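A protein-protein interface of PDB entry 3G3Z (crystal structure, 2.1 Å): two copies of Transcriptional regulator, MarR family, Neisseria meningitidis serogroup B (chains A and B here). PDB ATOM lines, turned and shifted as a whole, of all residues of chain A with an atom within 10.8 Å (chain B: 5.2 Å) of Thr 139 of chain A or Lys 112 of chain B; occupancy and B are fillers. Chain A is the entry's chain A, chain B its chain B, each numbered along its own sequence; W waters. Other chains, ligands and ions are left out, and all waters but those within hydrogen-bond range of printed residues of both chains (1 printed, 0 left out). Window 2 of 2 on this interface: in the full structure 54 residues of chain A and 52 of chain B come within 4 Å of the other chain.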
ATOM      1  N   ASN A   4     -17.260  -0.595  -5.541  1.00  0.00           N
ATOM      2  CA  ASN A   4     -17.709   0.166  -6.697  1.00  0.00           C
ATOM      3  C   ASN A   4     -19.203   0.465  -6.603  1.00  0.00           C
ATOM      4  O   ASN A   4     -19.984  -0.365  -6.140  1.00  0.00           O
ATOM      5  CB  ASN A   4     -17.388  -0.587  -7.987  1.00  0.00           C
ATOM      6  CG  ASN A   4     -17.730   0.203  -9.231  1.00  0.00           C
ATOM      7  OD1 ASN A   4     -18.443  -0.284 -10.100  1.00  0.00           O
ATOM      8  ND2 ASN A   4     -17.225   1.432  -9.318  1.00  0.00           N
ATOM      9  N   GLN A   5     -19.583   1.656  -7.042  1.00  0.00           N
ATOM     10  CA  GLN A   5     -20.958   2.129  -6.945  1.00  0.00           C
ATOM     11  C   GLN A   5     -21.915   1.206  -7.685  1.00  0.00           C
ATOM     12  O   GLN A   5     -22.967   0.838  -7.168  1.00  0.00           O
ATOM     13  CB  GLN A   5     -21.057   3.500  -7.581  1.00  0.00           C
ATOM     14  CG  GLN A   5     -21.718   4.513  -6.719  1.00  0.00           C
ATOM     15  CD  GLN A   5     -20.738   5.526  -6.228  1.00  0.00           C
ATOM     16  OE1 GLN A   5     -20.392   6.469  -6.945  1.00  0.00           O
ATOM     17  NE2 GLN A   5     -20.265   5.340  -5.003  1.00  0.00           N
ATOM     18  N   LEU A   6     -21.527   0.859  -8.908  1.00  0.00           N
ATOM     19  CA  LEU A   6     -22.308   0.016  -9.795  1.00  0.00           C
ATOM     20  C   LEU A   6     -22.482  -1.364  -9.187  1.00  0.00           C
ATOM     21  O   LEU A   6     -23.558  -1.958  -9.270  1.00  0.00           O
ATOM     22  CB  LEU A   6     -21.595  -0.086 -11.146  1.00  0.00           C
ATOM     23  CG  LEU A   6     -22.320  -0.305 -12.483  1.00  0.00           C
ATOM     24  CD1 LEU A   6     -21.844  -1.582 -13.194  1.00  0.00           C
ATOM     25  CD2 LEU A   6     -23.848  -0.218 -12.376  1.00  0.00           C
ATOM     26  N   LEU A   9     -24.872  -1.039  -6.307  1.00  0.00           N
ATOM     27  CA  LEU A   9     -26.235  -0.882  -6.808  1.00  0.00           C
ATOM     28  C   LEU A   9     -26.777  -2.205  -7.347  1.00  0.00           C
ATOM     29  O   LEU A   9     -27.885  -2.622  -6.997  1.00  0.00           O
ATOM     30  CB  LEU A   9     -26.311   0.209  -7.898  1.00  0.00           C
ATOM     31  CG  LEU A   9     -27.718   0.432  -8.481  1.00  0.00           C
ATOM     32  CD1 LEU A   9     -28.600   1.165  -7.472  1.00  0.00           C
ATOM     33  CD2 LEU A   9     -27.685   1.180  -9.802  1.00  0.00           C
ATOM     34  N   ALA A 131     -33.979   8.086 -11.385  1.00  0.00           N
ATOM     35  CA  ALA A 131     -32.859   8.819 -11.964  1.00  0.00           C
ATOM     36  C   ALA A 131     -31.778   7.876 -12.453  1.00  0.00           C
ATOM     37  O   ALA A 131     -31.243   8.055 -13.548  1.00  0.00           O
ATOM     38  CB  ALA A 131     -32.285   9.806 -10.955  1.00  0.00           C
ATOM     39  N   LEU A 132     -31.456   6.877 -11.638  1.00  0.00           N
ATOM     40  CA  LEU A 132     -30.440   5.899 -12.010  1.00  0.00           C
ATOM     41  C   LEU A 132     -30.850   5.142 -13.267  1.00  0.00           C
ATOM     42  O   LEU A 132     -30.073   5.056 -14.200  1.00  0.00           O
ATOM     43  CB  LEU A 132     -30.153   4.939 -10.858  1.00  0.00           C
ATOM     44  CG  LEU A 132     -29.307   5.548  -9.737  1.00  0.00           C
ATOM     45  CD1 LEU A 132     -29.497   4.777  -8.433  1.00  0.00           C
ATOM     46  CD2 LEU A 132     -27.834   5.627 -10.121  1.00  0.00           C
ATOM     47  N   ALA A 133     -32.084   4.642 -13.294  1.00  0.00           N
ATOM     48  CA  ALA A 133     -32.631   3.942 -14.454  1.00  0.00           C
ATOM     49  C   ALA A 133     -32.585   4.793 -15.729  1.00  0.00           C
ATOM     50  O   ALA A 133     -32.195   4.306 -16.786  1.00  0.00           O
ATOM     51  CB  ALA A 133     -34.066   3.448 -14.171  1.00  0.00           C
ATOM     52  N   GLU A 134     -32.980   6.059 -15.600  1.00  0.00           N
ATOM     53  CA  GLU A 134     -32.870   7.071 -16.652  1.00  0.00           C
ATOM     54  C   GLU A 134     -31.458   7.219 -17.250  1.00  0.00           C
ATOM     55  O   GLU A 134     -31.280   7.131 -18.464  1.00  0.00           O
ATOM     56  CB  GLU A 134     -33.378   8.411 -16.105  1.00  0.00           C
ATOM     57  CG  GLU A 134     -32.769   9.667 -16.727  1.00  0.00           C
ATOM     58  CD  GLU A 134     -33.371  10.020 -18.078  1.00  0.00           C
ATOM     59  OE1 GLU A 134     -34.507   9.573 -18.366  1.00  0.00           O
ATOM     60  OE2 GLU A 134     -32.710  10.757 -18.852  1.00  0.00           O
ATOM     61  N   VAL A 135     -30.467   7.454 -16.391  1.00  0.00           N
ATOM     62  CA  VAL A 135     -29.070   7.643 -16.817  1.00  0.00           C
ATOM     63  C   VAL A 135     -28.517   6.367 -17.438  1.00  0.00           C
ATOM     64  O   VAL A 135     -27.851   6.405 -18.480  1.00  0.00           O
ATOM     65  CB  VAL A 135     -28.147   8.052 -15.636  1.00  0.00           C
ATOM     66  CG1 VAL A 135     -26.735   8.279 -16.124  1.00  0.00           C
ATOM     67  CG2 VAL A 135     -28.658   9.311 -14.959  1.00  0.00           C
ATOM     68  N   MET A 136     -28.807   5.242 -16.791  1.00  0.00           N
ATOM     69  CA  MET A 136     -28.370   3.946 -17.284  1.00  0.00           C
ATOM     70  C   MET A 136     -28.918   3.668 -18.671  1.00  0.00           C
ATOM     71  O   MET A 136     -28.160   3.256 -19.540  1.00  0.00           O
ATOM     72  CB  MET A 136     -28.785   2.825 -16.338  1.00  0.00           C
ATOM     73  CG  MET A 136     -28.107   2.866 -15.004  1.00  0.00           C
ATOM     74  SD  MET A 136     -28.932   1.626 -13.741  1.00  0.00           S
ATOM     75  CE  MET A 136     -30.775   1.717 -14.316  1.00  0.00           C
ATOM     76  N   GLU A 137     -30.224   3.885 -18.878  1.00  0.00           N
ATOM     77  CA  GLU A 137     -30.843   3.673 -20.197  1.00  0.00           C
ATOM     78  C   GLU A 137     -30.166   4.535 -21.254  1.00  0.00           C
ATOM     79  O   GLU A 137     -29.820   4.058 -22.330  1.00  0.00           O
ATOM     80  CB  GLU A 137     -32.347   3.988 -20.188  1.00  0.00           C
ATOM     81  CG  GLU A 137     -33.238   2.928 -19.545  1.00  0.00           C
ATOM     82  CD  GLU A 137     -33.491   1.707 -20.436  1.00  0.00           C
ATOM     83  OE1 GLU A 137     -34.449   0.955 -20.142  1.00  0.00           O
ATOM     84  OE2 GLU A 137     -32.752   1.487 -21.425  1.00  0.00           O
ATOM     85  N   LYS A 138     -29.976   5.806 -20.920  1.00  0.00           N
ATOM     86  CA  LYS A 138     -29.409   6.797 -21.829  1.00  0.00           C
ATOM     87  C   LYS A 138     -27.958   6.471 -22.203  1.00  0.00           C
ATOM     88  O   LYS A 138     -27.563   6.624 -23.364  1.00  0.00           O
ATOM     89  CB  LYS A 138     -29.529   8.188 -21.191  1.00  0.00           C
ATOM     90  CG  LYS A 138     -28.815   9.332 -21.893  1.00  0.00           C
ATOM     91  CD  LYS A 138     -28.808  10.550 -20.968  1.00  0.00           C
ATOM     92  CE  LYS A 138     -27.989  11.693 -21.525  1.00  0.00           C
ATOM     93  NZ  LYS A 138     -28.783  12.480 -22.505  1.00  0.00           N
ATOM     94  N   THR A 139     -27.186   6.006 -21.221  1.00  0.00           N
ATOM     95  CA  THR A 139     -25.768   5.675 -21.413  1.00  0.00           C
ATOM     96  C   THR A 139     -25.600   4.425 -22.278  1.00  0.00           C
ATOM     97  O   THR A 139     -24.734   4.380 -23.158  1.00  0.00           O
ATOM     98  CB  THR A 139     -25.056   5.483 -20.055  1.00  0.00           C
ATOM     99  OG1 THR A 139     -25.221   6.668 -19.268  1.00  0.00           O
ATOM    100  CG2 THR A 139     -23.560   5.221 -20.238  1.00  0.00           C
ATOM    101  N   ILE A 140     -26.436   3.419 -22.014  1.00  0.00           N
ATOM    102  CA  ILE A 140     -26.488   2.190 -22.807  1.00  0.00           C
ATOM    103  C   ILE A 140     -26.881   2.511 -24.257  1.00  0.00           C
ATOM    104  O   ILE A 140     -26.321   1.936 -25.201  1.00  0.00           O
ATOM    105  CB  ILE A 140     -27.481   1.170 -22.200  1.00  0.00           C
ATOM    106  CG1 ILE A 140     -26.990   0.664 -20.834  1.00  0.00           C
ATOM    107  CG2 ILE A 140     -27.723  -0.010 -23.152  1.00  0.00           C
ATOM    108  CD1 ILE A 140     -28.081  -0.016 -20.001  1.00  0.00           C
ATOM    109  N   SER A 141     -27.844   3.420 -24.426  1.00  0.00           N
ATOM    110  CA  SER A 141     -28.238   3.898 -25.756  1.00  0.00           C
ATOM    111  C   SER A 141     -27.063   4.544 -26.477  1.00  0.00           C
ATOM    112  O   SER A 141     -26.782   4.217 -27.628  1.00  0.00           O
ATOM    113  CB  SER A 141     -29.398   4.890 -25.662  1.00  0.00           C
ATOM    114  OG  SER A 141     -30.616   4.217 -25.404  1.00  0.00           O
ATOM    115  N   GLU A 142     -26.366   5.445 -25.791  1.00  0.00           N
ATOM    116  CA  GLU A 142     -25.181   6.084 -26.359  1.00  0.00           C
ATOM    117  C   GLU A 142     -24.102   5.080 -26.743  1.00  0.00           C
ATOM    118  O   GLU A 142     -23.522   5.174 -27.821  1.00  0.00           O
ATOM    119  CB  GLU A 142     -24.610   7.126 -25.400  1.00  0.00           C
ATOM    120  CG  GLU A 142     -25.449   8.391 -25.334  1.00  0.00           C
ATOM    121  CD  GLU A 142     -25.234   9.173 -24.055  1.00  0.00           C
ATOM    122  OE1 GLU A 142     -24.465   8.700 -23.185  1.00  0.00           O
ATOM    123  OE2 GLU A 142     -25.840  10.259 -23.921  1.00  0.00           O
ATOM    124  N   ASN A 143     -23.851   4.112 -25.869  1.00  0.00           N
ATOM    125  CA  ASN A 143     -22.785   3.130 -26.085  1.00  0.00           C
ATOM    126  C   ASN A 143     -23.009   2.214 -27.293  1.00  0.00           C
ATOM    127  O   ASN A 143     -22.117   1.463 -27.681  1.00  0.00           O
ATOM    128  CB  ASN A 143     -22.538   2.318 -24.811  1.00  0.00           C
ATOM    129  CG  ASN A 143     -22.047   3.177 -23.669  1.00  0.00           C
ATOM    130  OD1 ASN A 143     -21.870   4.386 -23.823  1.00  0.00           O
ATOM    131  ND2 ASN A 143     -21.835   2.566 -22.513  1.00  0.00           N
ATOM    132  N   LYS A 144     -24.204   2.283 -27.872  1.00  0.00           N
ATOM    133  CA  LYS A 144     -24.488   1.627 -29.136  1.00  0.00           C
ATOM    134  C   LYS A 144     -24.097   2.561 -30.267  1.00  0.00           C
ATOM    135  O   LYS A 144     -23.146   2.295 -30.995  1.00  0.00           O
ATOM    136  CB  LYS A 144     -25.971   1.296 -29.253  1.00  0.00           C
ATOM    137  CG  LYS A 144     -26.494   0.326 -28.221  1.00  0.00           C
ATOM    138  CD  LYS A 144     -27.941  -0.004 -28.515  1.00  0.00           C
ATOM    139  CE  LYS A 144     -28.605  -0.664 -27.318  1.00  0.00           C
ATOM    140  NZ  LYS A 144     -30.069  -0.800 -27.544  1.00  0.00           N
ATOM    141  N   GLN B 107     -16.377   0.425 -14.508  1.00  0.00           N
ATOM    142  CA  GLN B 107     -15.993   1.665 -13.831  1.00  0.00           C
ATOM    143  C   GLN B 107     -16.455   2.875 -14.625  1.00  0.00           C
ATOM    144  O   GLN B 107     -16.939   3.860 -14.054  1.00  0.00           O
ATOM    145  CB  GLN B 107     -14.480   1.728 -13.628  1.00  0.00           C
ATOM    146  CG  GLN B 107     -14.025   2.820 -12.671  1.00  0.00           C
ATOM    147  CD  GLN B 107     -14.576   2.632 -11.266  1.00  0.00           C
ATOM    148  OE1 GLN B 107     -14.299   1.629 -10.604  1.00  0.00           O
ATOM    149  NE2 GLN B 107     -15.351   3.605 -10.801  1.00  0.00           N
ATOM    150  N   GLU B 108     -16.307   2.781 -15.943  1.00  0.00           N
ATOM    151  CA  GLU B 108     -16.757   3.807 -16.866  1.00  0.00           C
ATOM    152  C   GLU B 108     -18.257   4.046 -16.721  1.00  0.00           C
ATOM    153  O   GLU B 108     -18.693   5.178 -16.478  1.00  0.00           O
ATOM    154  CB  GLU B 108     -16.418   3.390 -18.292  1.00  0.00           C
ATOM    155  CG  GLU B 108     -16.502   4.506 -19.318  1.00  0.00           C
ATOM    156  CD  GLU B 108     -15.556   4.282 -20.484  1.00  0.00           C
ATOM    157  OE1 GLU B 108     -14.856   3.240 -20.489  1.00  0.00           O
ATOM    158  OE2 GLU B 108     -15.504   5.147 -21.390  1.00  0.00           O
ATOM    159  N   PHE B 109     -19.032   2.969 -16.858  1.00  0.00           N
ATOM    160  CA  PHE B 109     -20.494   3.012 -16.721  1.00  0.00           C
ATOM    161  C   PHE B 109     -20.869   3.536 -15.344  1.00  0.00           C
ATOM    162  O   PHE B 109     -21.756   4.367 -15.225  1.00  0.00           O
ATOM    163  CB  PHE B 109     -21.090   1.613 -16.950  1.00  0.00           C
ATOM    164  CG  PHE B 109     -22.609   1.568 -17.004  1.00  0.00           C
ATOM    165  CD1 PHE B 109     -23.320   2.223 -18.021  1.00  0.00           C
ATOM    166  CD2 PHE B 109     -23.327   0.820 -16.067  1.00  0.00           C
ATOM    167  CE1 PHE B 109     -24.726   2.162 -18.082  1.00  0.00           C
ATOM    168  CE2 PHE B 109     -24.737   0.751 -16.120  1.00  0.00           C
ATOM    169  CZ  PHE B 109     -25.435   1.423 -17.140  1.00  0.00           C
ATOM    170  N   SER B 110     -20.178   3.056 -14.313  1.00  0.00           N
ATOM    171  CA  SER B 110     -20.409   3.505 -12.935  1.00  0.00           C
ATOM    172  C   SER B 110     -20.213   5.011 -12.744  1.00  0.00           C
ATOM    173  O   SER B 110     -20.956   5.648 -11.987  1.00  0.00           O
ATOM    174  CB  SER B 110     -19.502   2.741 -11.968  1.00  0.00           C
ATOM    175  OG  SER B 110     -19.827   3.037 -10.625  1.00  0.00           O
ATOM    176  N   ASP B 111     -19.213   5.569 -13.423  1.00  0.00           N
ATOM    177  CA  ASP B 111     -18.874   6.976 -13.276  1.00  0.00           C
ATOM    178  C   ASP B 111     -19.904   7.864 -13.953  1.00  0.00           C
ATOM    179  O   ASP B 111     -20.385   8.815 -13.346  1.00  0.00           O
ATOM    180  CB  ASP B 111     -17.468   7.261 -13.795  1.00  0.00           C
ATOM    181  CG  ASP B 111     -16.390   6.672 -12.906  1.00  0.00           C
ATOM    182  OD1 ASP B 111     -16.708   6.150 -11.811  1.00  0.00           O
ATOM    183  OD2 ASP B 111     -15.212   6.719 -13.306  1.00  0.00           O
ATOM    184  N   LYS B 112     -20.252   7.542 -15.196  1.00  0.00           N
ATOM    185  CA  LYS B 112     -21.300   8.278 -15.903  1.00  0.00           C
ATOM    186  C   LYS B 112     -22.594   8.217 -15.109  1.00  0.00           C
ATOM    187  O   LYS B 112     -23.273   9.226 -14.929  1.00  0.00           O
ATOM    188  CB  LYS B 112     -21.554   7.702 -17.296  1.00  0.00           C
ATOM    189  CG  LYS B 112     -20.326   7.531 -18.152  1.00  0.00           C
ATOM    190  CD  LYS B 112     -20.717   7.248 -19.588  1.00  0.00           C
ATOM    191  CE  LYS B 112     -19.764   6.262 -20.258  1.00  0.00           C
ATOM    192  NZ  LYS B 112     -19.935   4.865 -19.737  1.00  0.00           N
ATOM    193  N   VAL B 113     -22.905   7.025 -14.614  1.00  0.00           N
ATOM    194  CA  VAL B 113     -24.206   6.733 -14.028  1.00  0.00           C
ATOM    195  C   VAL B 113     -24.458   7.476 -12.708  1.00  0.00           C
ATOM    196  O   VAL B 113     -25.563   7.979 -12.483  1.00  0.00           O
ATOM    197  CB  VAL B 113     -24.424   5.196 -13.912  1.00  0.00           C
ATOM    198  CG1 VAL B 113     -25.444   4.833 -12.840  1.00  0.00           C
ATOM    199  CG2 VAL B 113     -24.830   4.627 -15.270  1.00  0.00           C
ATOM    200  N   PHE B 114     -23.428   7.564 -11.867  1.00  0.00           N
ATOM    201  CA  PHE B 114     -23.560   8.198 -10.558  1.00  0.00           C
ATOM    202  C   PHE B 114     -23.123   9.665 -10.528  1.00  0.00           C
ATOM    203  O   PHE B 114     -23.089  10.292  -9.463  1.00  0.00           O
ATOM    204  CB  PHE B 114     -22.843   7.362  -9.490  1.00  0.00           C
ATOM    205  CG  PHE B 114     -23.521   6.055  -9.217  1.00  0.00           C
ATOM    206  CD1 PHE B 114     -24.509   5.964  -8.242  1.00  0.00           C
ATOM    207  CD2 PHE B 114     -23.211   4.923  -9.968  1.00  0.00           C
ATOM    208  CE1 PHE B 114     -25.158   4.757  -7.999  1.00  0.00           C
ATOM    209  CE2 PHE B 114     -23.856   3.714  -9.733  1.00  0.00           C
ATOM    210  CZ  PHE B 114     -24.830   3.632  -8.747  1.00  0.00           C
ATOM    211  N   ALA B 115     -22.838  10.214 -11.705  1.00  0.00           N
ATOM    212  CA  ALA B 115     -22.434  11.613 -11.844  1.00  0.00           C
ATOM    213  C   ALA B 115     -23.238  12.586 -10.965  1.00  0.00           C
ATOM    214  O   ALA B 115     -22.651  13.410 -10.264  1.00  0.00           O
ATOM    215  CB  ALA B 115     -22.476  12.041 -13.314  1.00  0.00           C
HETATM  216  O   HOH W   1     -21.497   9.546  -6.929  1.00  0.00           O
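The side-chain hydroxyl (OG) of Ser 110 of chain B is in hydrogen-bond range of the backbone NH (N) of Leu 6 of chain A (3.3 Å). OE1 of Gln 107 of chain B lies within hydrogen-bond range of ND2 of Asn 4 of chain A (3.2 Å). The side-chain hydroxyl of Ser 110 of chain B is in hydrogen-bond range of the side-chain amide nitrogen of Asn 4 of chain A (3.3 Å).
The side-chain amide nitrogen (NE2) of Gln 107 of chain B sits at hydrogen-bond distance from the side-chain carboxylate (OD1) of Asp 111 of chain B, at 3.1 Å. OD1 of Asn 143 of chain A lies close to O of Thr 139 of chain A. OG1 of Thr 139 of chain A lies within hydrogen-bond range of O of Val 135 of chain A (2.8 Å). The side-chain amide oxygen (OD1) of Asn 4 of chain A sits close to the backbone NH (N) of Leu 6 of chain A.
Ser 110 of chain B touches Gln 5 of chain A. CG of Gln 5 of chain A touches CG of Phe 114 of chain B, 3.4 Å away. Leu 6 of chain A touches Phe 109 of chain B (CD2 to CD2, 3.9 Å). Leu 9 of chain A touches Phe 114 of chain B. Val 113 of chain B touches Leu 132 of chain A (CG1 to CD2, 3.7 Å). CD2 of Leu 132 of chain A touches CE1 of Phe 114 of chain B, 3.5 Å away. Lys 112 of chain B touches Val 135 of chain A. CG1 of Val 135 of chain A touches CA of Val 113 of chain B (3.6 Å). Met 136 of chain A touches Phe 109 of chain B (CG to CZ, 3.7 Å). Phe 109 of chain B touches Thr 139 of chain A (CD1 to CG2, 3.7 Å).
No position is printed for both chains.
Water W1 bridges the backbone carbonyl oxygen (O) of Phe 114 of chain B (3.1 Å) and the side-chain amide oxygen (OE1) of Gln 5 of chain A (3.3 Å).
Printed residues of chain B that touch a printed residue of chain A: Gln 107, Phe 109, Ser 110, Lys 112, Val 113 and Phe 114. Hydrophobic or aromatic side chains of chain B that line the printed part of chain A: Phe 109, Val 113 and Phe 114. Of the 18 printed residues of chain A, 9 touch a printed residue of chain B. Hydrophobic or aromatic side chains of chain A that line the printed part of chain B: Leu 6, Leu 9, Leu 132, Val 135, Met 136 and Ile 140. Among the printed residues, no Asp or Glu carboxylate lies within 4 Å of a Lys or Arg side-chain nitrogen of the other chain.
Printed residues of chain B within 4 Å of Asn 4 of chain A: Gln 107 and Ser 110. Ala 133 of chain A touches none of the printed residues of chain B. Glu 137 of chain A touches none of the printed residues of chain B. Thr 139 of chain A touches just these residues of chain B: Phe 109 (3.7 Å) and Lys 112 (3.6 Å). Of chain A, only Leu 6 (3.9 Å), Met 136 (3.7 Å), Thr 139 (3.7 Å) and Ile 140 (3.9 Å) come within 4 Å of Phe 109 of chain B. Of the printed residues of chain A, Ser 110 of chain B touches Asn 4, Gln 5 and Leu 6. No residue of chain A comes within 4 Å of Asp 111 of chain B. Lys 112 of chain B touches just these residues of chain A: Val 135 (3.8 Å) and Thr 139 (3.6 Å). Of chain A, only Leu 132 (3.7 Å), Val 135 (3.6 Å) and Met 136 (3.7 Å) come within 4 Å of Val 113 of chain B. Printed residues of chain A within 4 Å of Phe 114 of chain B: Gln 5 (3.4 Å), Leu 6 (3.8 Å), Leu 9 (3.8 Å) and Leu 132 (3.5 Å). No residue of chain A comes within 4 Å of Ala 115 of chain B. The nearest residue of chain A that does not touch Lys 112 of chain B is Asn 143 of chain A (4.1 Å). The nearest printed residue of chain B that does not touch Leu 9 of chain A is Val 113 of chain B (5.3 Å).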
